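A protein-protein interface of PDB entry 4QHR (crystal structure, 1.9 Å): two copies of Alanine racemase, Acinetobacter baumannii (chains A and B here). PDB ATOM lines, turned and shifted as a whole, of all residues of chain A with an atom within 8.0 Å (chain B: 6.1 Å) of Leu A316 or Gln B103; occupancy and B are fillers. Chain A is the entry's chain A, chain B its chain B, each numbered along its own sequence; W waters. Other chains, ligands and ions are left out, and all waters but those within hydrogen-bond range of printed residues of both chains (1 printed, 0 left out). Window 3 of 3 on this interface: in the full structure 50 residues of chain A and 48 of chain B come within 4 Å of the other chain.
O of Ile A268 is in hydrogen-bond range of N of Ile A241 (2.7 Å).
Phe B82 touches Ile A241. Ile A241 touches His B101. His B101 touches Leu A316. Gln B103 touches Leu A316.
Of the printed residues of chain B, Ile A241 touches Phe B82 (3.7 Å) and His B101 (3.1 Å). Ile A268 touches none of the printed residues of chain B. Of chain B, only His B101 (3.7 Å) and Gln B103 (3.6 Å) come within 4 Å of Leu A316. Printed residues of chain A within 4 Å of His B101: Ile A241 (3.1 Å) and Leu A316 (3.7 Å). Gln B103 touches just one residue of chain A: Leu A316. The nearest printed residue of chain B that does not touch Leu A316 is Gln B102 (7.0 Å).
Of the 14 printed residues of chain A, 2 touch a printed residue of chain B. Printed residues of chain A that touch a printed residue of chain B: Ile A241 and Leu A316. Hydrophobic or aromatic side chains of chain A within 4 Å of the printed part of chain B: Ile A241 and Leu A316. Along chain A the printed residues that touch a printed residue of chain B span positions 241 to 316. Of the 11 printed residues of chain B, 3 touch a printed residue of chain A. Hydrophobic or aromatic side chains of chain B that line the printed part of chain A: Phe B82 and His B101. Along chain B the printed residues that touch a printed residue of chain A span positions 82 to 103. Among the printed residues, 4 pairs touch across the chains.
No position is printed for both chains.
Water W1 lies within hydrogen-bond range of ND1 of His B101 (2.8 Å) and N of Leu A243 (3.0 Å).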
ATOM      1  N   GLU A 239      15.917   7.916  -4.361  1.00  0.00           N
ATOM      2  CA  GLU A 239      16.517   9.185  -3.985  1.00  0.00           C
ATOM      3  C   GLU A 239      15.512  10.317  -4.021  1.00  0.00           C
ATOM      4  O   GLU A 239      14.464  10.280  -4.710  1.00  0.00           O
ATOM      5  CB  GLU A 239      17.723   9.527  -4.920  1.00  0.00           C
ATOM      6  CG  GLU A 239      18.998   8.778  -4.540  1.00  0.00           C
ATOM      7  CD  GLU A 239      20.141   9.122  -5.461  1.00  0.00           C
ATOM      8  OE1 GLU A 239      20.015  10.126  -6.234  1.00  0.00           O
ATOM      9  OE2 GLU A 239      21.148   8.401  -5.412  1.00  0.00           O
ATOM     10  N   ILE A 240      15.847  11.330  -3.244  1.00  0.00           N
ATOM     11  CA  ILE A 240      15.109  12.599  -3.286  1.00  0.00           C
ATOM     12  C   ILE A 240      15.340  13.362  -4.588  1.00  0.00           C
ATOM     13  O   ILE A 240      16.459  13.644  -4.949  1.00  0.00           O
ATOM     14  CB  ILE A 240      15.418  13.469  -2.069  1.00  0.00           C
ATOM     15  CG1 ILE A 240      14.791  12.783  -0.859  1.00  0.00           C
ATOM     16  CG2 ILE A 240      14.825  14.865  -2.282  1.00  0.00           C
ATOM     17  CD1 ILE A 240      15.121  13.399   0.494  1.00  0.00           C
ATOM     18  N   ILE A 241      14.255  13.693  -5.276  1.00  0.00           N
ATOM     19  CA  ILE A 241      14.307  14.365  -6.580  1.00  0.00           C
ATOM     20  C   ILE A 241      13.773  15.797  -6.573  1.00  0.00           C
ATOM     21  O   ILE A 241      13.969  16.530  -7.552  1.00  0.00           O
ATOM     22  CB  ILE A 241      13.604  13.520  -7.668  1.00  0.00           C
ATOM     23  CG1 ILE A 241      12.119  13.279  -7.378  1.00  0.00           C
ATOM     24  CG2 ILE A 241      14.312  12.173  -7.795  1.00  0.00           C
ATOM     25  CD1 ILE A 241      11.325  12.721  -8.555  1.00  0.00           C
ATOM     26  N   ALA A 242      13.075  16.171  -5.499  1.00  0.00           N
ATOM     27  CA  ALA A 242      12.550  17.526  -5.326  1.00  0.00           C
ATOM     28  C   ALA A 242      12.308  17.859  -3.866  1.00  0.00           C
ATOM     29  O   ALA A 242      11.956  16.984  -3.075  1.00  0.00           O
ATOM     30  CB  ALA A 242      11.247  17.730  -6.104  1.00  0.00           C
ATOM     31  N   LEU A 243      12.488  19.145  -3.530  1.00  0.00           N
ATOM     32  CA  LEU A 243      12.218  19.645  -2.203  1.00  0.00           C
ATOM     33  C   LEU A 243      11.204  20.777  -2.249  1.00  0.00           C
ATOM     34  O   LEU A 243      11.241  21.602  -3.171  1.00  0.00           O
ATOM     35  CB  LEU A 243      13.517  20.134  -1.570  1.00  0.00           C
ATOM     36  CG  LEU A 243      14.441  18.961  -1.294  1.00  0.00           C
ATOM     37  CD1 LEU A 243      15.821  19.471  -0.972  1.00  0.00           C
ATOM     38  CD2 LEU A 243      13.894  18.121  -0.142  1.00  0.00           C
ATOM     39  N   ASN A 244      10.328  20.836  -1.254  1.00  0.00           N
ATOM     40  CA  ASN A 244       9.218  21.757  -1.307  1.00  0.00           C
ATOM     41  C   ASN A 244       8.850  22.211   0.088  1.00  0.00           C
ATOM     42  O   ASN A 244       8.627  21.390   0.954  1.00  0.00           O
ATOM     43  CB  ASN A 244       8.063  21.040  -2.027  1.00  0.00           C
ATOM     44  CG  ASN A 244       6.841  21.899  -2.276  1.00  0.00           C
ATOM     45  OD1 ASN A 244       5.705  21.387  -2.307  1.00  0.00           O
ATOM     46  ND2 ASN A 244       7.032  23.183  -2.475  1.00  0.00           N
ATOM     47  N   ALA A 267       9.728  16.194   0.731  1.00  0.00           N
ATOM     48  CA  ALA A 267      10.616  15.767  -0.357  1.00  0.00           C
ATOM     49  C   ALA A 267       9.852  14.794  -1.279  1.00  0.00           C
ATOM     50  O   ALA A 267       9.025  14.008  -0.818  1.00  0.00           O
ATOM     51  CB  ALA A 267      11.834  15.102   0.206  1.00  0.00           C
ATOM     52  N   ILE A 268      10.158  14.868  -2.572  1.00  0.00           N
ATOM     53  CA  ILE A 268       9.657  13.911  -3.512  1.00  0.00           C
ATOM     54  C   ILE A 268      10.761  12.884  -3.767  1.00  0.00           C
ATOM     55  O   ILE A 268      11.948  13.219  -3.966  1.00  0.00           O
ATOM     56  CB  ILE A 268       9.159  14.558  -4.808  1.00  0.00           C
ATOM     57  CG1 ILE A 268       8.159  15.678  -4.510  1.00  0.00           C
ATOM     58  CG2 ILE A 268       8.546  13.497  -5.725  1.00  0.00           C
ATOM     59  CD1 ILE A 268       6.949  15.260  -3.681  1.00  0.00           C
ATOM     60  N   VAL A 314      18.183  16.813   4.676  1.00  0.00           N
ATOM     61  CA  VAL A 314      18.233  16.134   3.405  1.00  0.00           C
ATOM     62  C   VAL A 314      18.680  17.104   2.340  1.00  0.00           C
ATOM     63  O   VAL A 314      18.736  18.324   2.568  1.00  0.00           O
ATOM     64  CB  VAL A 314      16.862  15.550   2.984  1.00  0.00           C
ATOM     65  CG1 VAL A 314      16.385  14.513   3.997  1.00  0.00           C
ATOM     66  CG2 VAL A 314      15.830  16.664   2.774  1.00  0.00           C
ATOM     67  N   LYS A 315      19.017  16.535   1.198  1.00  0.00           N
ATOM     68  CA  LYS A 315      19.314  17.283   0.029  1.00  0.00           C
ATOM     69  C   LYS A 315      18.762  16.559  -1.181  1.00  0.00           C
ATOM     70  O   LYS A 315      18.333  15.404  -1.093  1.00  0.00           O
ATOM     71  CB  LYS A 315      20.821  17.412  -0.151  1.00  0.00           C
ATOM     72  CG  LYS A 315      21.517  18.325   0.846  1.00  0.00           C
ATOM     73  CD  LYS A 315      22.954  18.532   0.415  1.00  0.00           C
ATOM     74  CE  LYS A 315      23.200  19.398  -0.811  1.00  0.00           C
ATOM     75  NZ  LYS A 315      23.031  20.838  -0.485  1.00  0.00           N
ATOM     76  N   LEU A 316      18.806  17.237  -2.319  1.00  0.00           N
ATOM     77  CA  LEU A 316      18.571  16.602  -3.610  1.00  0.00           C
ATOM     78  C   LEU A 316      19.643  15.507  -3.749  1.00  0.00           C
ATOM     79  O   LEU A 316      20.822  15.737  -3.464  1.00  0.00           O
ATOM     80  CB  LEU A 316      18.618  17.618  -4.766  1.00  0.00           C
ATOM     81  CG  LEU A 316      17.481  18.647  -4.813  1.00  0.00           C
ATOM     82  CD1 LEU A 316      17.754  19.661  -5.906  1.00  0.00           C
ATOM     83  CD2 LEU A 316      16.107  18.003  -5.028  1.00  0.00           C
ATOM     84  N   GLY A 317      19.212  14.291  -4.102  1.00  0.00           N
ATOM     85  CA  GLY A 317      20.118  13.145  -4.207  1.00  0.00           C
ATOM     86  C   GLY A 317      20.227  12.311  -2.953  1.00  0.00           C
ATOM     87  O   GLY A 317      20.854  11.261  -2.998  1.00  0.00           O
ATOM     88  N   THR A 318      19.662  12.757  -1.840  1.00  0.00           N
ATOM     89  CA  THR A 318      19.745  11.987  -0.593  1.00  0.00           C
ATOM     90  C   THR A 318      19.029  10.654  -0.782  1.00  0.00           C
ATOM     91  O   THR A 318      17.955  10.611  -1.384  1.00  0.00           O
ATOM     92  CB  THR A 318      19.088  12.715   0.556  1.00  0.00           C
ATOM     93  OG1 THR A 318      19.920  13.806   0.938  1.00  0.00           O
ATOM     94  CG2 THR A 318      18.796  11.838   1.735  1.00  0.00           C
ATOM     95  N   GLN A 319      19.675   9.615  -0.251  1.00  0.00           N
ATOM     96  CA  GLN A 319      19.284   8.241  -0.431  1.00  0.00           C
ATOM     97  C   GLN A 319      18.177   7.957   0.554  1.00  0.00           C
ATOM     98  O   GLN A 319      18.228   8.385   1.641  1.00  0.00           O
ATOM     99  CB  GLN A 319      20.477   7.276  -0.227  1.00  0.00           C
ATOM    100  CG  GLN A 319      21.115   6.798  -1.541  1.00  0.00           C
ATOM    101  CD  GLN A 319      21.631   5.358  -1.432  1.00  0.00           C
ATOM    102  OE1 GLN A 319      22.776   5.152  -1.029  1.00  0.00           O
ATOM    103  NE2 GLN A 319      20.781   4.343  -1.801  1.00  0.00           N
ATOM    104  N   VAL B  81      15.236  15.389 -16.312  1.00  0.00           N
ATOM    105  CA  VAL B  81      16.420  14.556 -16.050  1.00  0.00           C
ATOM    106  C   VAL B  81      16.825  14.632 -14.587  1.00  0.00           C
ATOM    107  O   VAL B  81      16.644  15.660 -13.959  1.00  0.00           O
ATOM    108  CB  VAL B  81      17.641  14.926 -16.903  1.00  0.00           C
ATOM    109  CG1 VAL B  81      17.391  14.637 -18.365  1.00  0.00           C
ATOM    110  CG2 VAL B  81      18.073  16.399 -16.662  1.00  0.00           C
ATOM    111  N   PHE B  82      17.399  13.552 -14.080  1.00  0.00           N
ATOM    112  CA  PHE B  82      17.755  13.412 -12.633  1.00  0.00           C
ATOM    113  C   PHE B  82      19.183  13.782 -12.326  1.00  0.00           C
ATOM    114  O   PHE B  82      19.512  14.125 -11.190  1.00  0.00           O
ATOM    115  CB  PHE B  82      17.442  11.975 -12.179  1.00  0.00           C
ATOM    116  CG  PHE B  82      16.023  11.599 -12.375  1.00  0.00           C
ATOM    117  CD1 PHE B  82      15.567  11.155 -13.602  1.00  0.00           C
ATOM    118  CD2 PHE B  82      15.118  11.734 -11.340  1.00  0.00           C
ATOM    119  CE1 PHE B  82      14.229  10.811 -13.784  1.00  0.00           C
ATOM    120  CE2 PHE B  82      13.795  11.392 -11.502  1.00  0.00           C
ATOM    121  CZ  PHE B  82      13.345  10.932 -12.728  1.00  0.00           C
ATOM    122  N   SER B  83      20.053  13.707 -13.331  1.00  0.00           N
ATOM    123  CA  SER B  83      21.432  14.120 -13.246  1.00  0.00           C
ATOM    124  C   SER B  83      21.854  14.836 -14.517  1.00  0.00           C
ATOM    125  O   SER B  83      21.363  14.570 -15.624  1.00  0.00           O
ATOM    126  CB  SER B  83      22.350  12.924 -12.960  1.00  0.00           C
ATOM    127  OG  SER B  83      22.325  11.967 -13.992  1.00  0.00           O
ATOM    128  N   HIS B 101      12.221  22.150 -11.408  1.00  0.00           N
ATOM    129  CA  HIS B 101      12.936  22.886 -10.382  1.00  0.00           C
ATOM    130  C   HIS B 101      14.239  23.521 -10.899  1.00  0.00           C
ATOM    131  O   HIS B 101      14.722  23.250 -12.024  1.00  0.00           O
ATOM    132  CB  HIS B 101      13.137  22.037  -9.106  1.00  0.00           C
ATOM    133  CG  HIS B 101      14.012  20.835  -9.287  1.00  0.00           C
ATOM    134  ND1 HIS B 101      14.572  20.170  -8.220  1.00  0.00           N
ATOM    135  CD2 HIS B 101      14.433  20.184 -10.396  1.00  0.00           C
ATOM    136  CE1 HIS B 101      15.287  19.155  -8.662  1.00  0.00           C
ATOM    137  NE2 HIS B 101      15.226  19.147  -9.981  1.00  0.00           N
ATOM    138  N   GLN B 102      14.789  24.399 -10.065  1.00  0.00           N
ATOM    139  CA  GLN B 102      15.943  25.227 -10.437  1.00  0.00           C
ATOM    140  C   GLN B 102      17.143  24.424 -10.934  1.00  0.00           C
ATOM    141  O   GLN B 102      17.846  24.817 -11.858  1.00  0.00           O
ATOM    142  CB  GLN B 102      16.409  26.062  -9.231  1.00  0.00           C
ATOM    143  CG  GLN B 102      17.359  27.199  -9.558  1.00  0.00           C
ATOM    144  CD  GLN B 102      16.765  28.238 -10.495  1.00  0.00           C
ATOM    145  OE1 GLN B 102      15.550  28.395 -10.635  1.00  0.00           O
ATOM    146  NE2 GLN B 102      17.636  28.959 -11.149  1.00  0.00           N
ATOM    147  N   GLN B 103      17.416  23.315 -10.287  1.00  0.00           N
ATOM    148  CA  GLN B 103      18.522  22.486 -10.753  1.00  0.00           C
ATOM    149  C   GLN B 103      18.426  22.109 -12.278  1.00  0.00           C
ATOM    150  O   GLN B 103      19.404  22.239 -13.064  1.00  0.00           O
ATOM    151  CB  GLN B 103      18.531  21.259  -9.875  1.00  0.00           C
ATOM    152  CG  GLN B 103      19.468  20.210 -10.305  1.00  0.00           C
ATOM    153  CD  GLN B 103      19.505  19.132  -9.304  1.00  0.00           C
ATOM    154  OE1 GLN B 103      20.285  19.200  -8.396  1.00  0.00           O
ATOM    155  NE2 GLN B 103      18.668  18.111  -9.469  1.00  0.00           N
ATOM    156  N   GLN B 104      17.259  21.674 -12.712  1.00  0.00           N
ATOM    157  CA  GLN B 104      17.087  21.291 -14.091  1.00  0.00           C
ATOM    158  C   GLN B 104      17.155  22.501 -14.997  1.00  0.00           C
ATOM    159  O   GLN B 104      17.617  22.379 -16.143  1.00  0.00           O
ATOM    160  CB  GLN B 104      15.766  20.551 -14.304  1.00  0.00           C
ATOM    161  CG  GLN B 104      15.751  19.166 -13.687  1.00  0.00           C
ATOM    162  CD  GLN B 104      14.351  18.595 -13.645  1.00  0.00           C
ATOM    163  OE1 GLN B 104      13.407  19.342 -13.581  1.00  0.00           O
ATOM    164  NE2 GLN B 104      14.219  17.263 -13.697  1.00  0.00           N
ATOM    165  N   PHE B 105      16.680  23.647 -14.528  1.00  0.00           N
ATOM    166  CA  PHE B 105      16.726  24.853 -15.363  1.00  0.00           C
ATOM    167  C   PHE B 105      18.189  25.206 -15.661  1.00  0.00           C
ATOM    168  O   PHE B 105      18.564  25.439 -16.806  1.00  0.00           O
ATOM    169  CB  PHE B 105      15.924  25.999 -14.724  1.00  0.00           C
ATOM    170  CG  PHE B 105      16.134  27.326 -15.375  1.00  0.00           C
ATOM    171  CD1 PHE B 105      15.448  27.661 -16.528  1.00  0.00           C
ATOM    172  CD2 PHE B 105      17.014  28.239 -14.838  1.00  0.00           C
ATOM    173  CE1 PHE B 105      15.622  28.881 -17.150  1.00  0.00           C
ATOM    174  CE2 PHE B 105      17.209  29.482 -15.462  1.00  0.00           C
ATOM    175  CZ  PHE B 105      16.498  29.797 -16.619  1.00  0.00           C
ATOM    176  N   GLU B 106      19.022  25.157 -14.635  1.00  0.00           N
ATOM    177  CA  GLU B 106      20.479  25.406 -14.753  1.00  0.00           C
ATOM    178  C   GLU B 106      21.138  24.442 -15.719  1.00  0.00           C
ATOM    179  O   GLU B 106      21.902  24.870 -16.591  1.00  0.00           O
ATOM    180  CB  GLU B 106      21.125  25.325 -13.343  1.00  0.00           C
ATOM    181  CG  GLU B 106      20.629  26.437 -12.423  1.00  0.00           C
ATOM    182  CD  GLU B 106      21.096  26.322 -10.974  1.00  0.00           C
ATOM    183  OE1 GLU B 106      21.582  25.246 -10.536  1.00  0.00           O
ATOM    184  OE2 GLU B 106      20.954  27.326 -10.234  1.00  0.00           O
ATOM    185  N   TRP B 107      20.823  23.149 -15.632  1.00  0.00           N
ATOM    186  CA  TRP B 107      21.437  22.170 -16.549  1.00  0.00           C
ATOM    187  C   TRP B 107      20.953  22.399 -17.983  1.00  0.00           C
ATOM    188  O   TRP B 107      21.720  22.253 -18.919  1.00  0.00           O
ATOM    189  CB  TRP B 107      21.167  20.715 -16.157  1.00  0.00           C
ATOM    190  CG  TRP B 107      21.652  20.319 -14.825  1.00  0.00           C
ATOM    191  CD1 TRP B 107      22.676  20.871 -14.122  1.00  0.00           C
ATOM    192  CD2 TRP B 107      21.126  19.264 -14.009  1.00  0.00           C
ATOM    193  NE1 TRP B 107      22.810  20.249 -12.914  1.00  0.00           N
ATOM    194  CE2 TRP B 107      21.882  19.247 -12.816  1.00  0.00           C
ATOM    195  CE3 TRP B 107      20.071  18.349 -14.157  1.00  0.00           C
ATOM    196  CZ2 TRP B 107      21.626  18.354 -11.773  1.00  0.00           C
ATOM    197  CZ3 TRP B 107      19.818  17.430 -13.085  1.00  0.00           C
ATOM    198  CH2 TRP B 107      20.598  17.454 -11.926  1.00  0.00           C
ATOM    199  N   LEU B 108      19.694  22.761 -18.154  1.00  0.00           N
ATOM    200  CA  LEU B 108      19.173  23.067 -19.497  1.00  0.00           C
ATOM    201  C   LEU B 108      19.856  24.292 -20.182  1.00  0.00           C
ATOM    202  O   LEU B 108      20.261  24.205 -21.357  1.00  0.00           O
ATOM    203  CB  LEU B 108      17.671  23.292 -19.437  1.00  0.00           C
ATOM    204  CG  LEU B 108      16.961  23.594 -20.755  1.00  0.00           C
ATOM    205  CD1 LEU B 108      17.021  22.436 -21.745  1.00  0.00           C
ATOM    206  CD2 LEU B 108      15.506  23.984 -20.494  1.00  0.00           C
HETATM  207  O   HOH W   1      13.640  20.871  -5.705  1.00  0.00           O
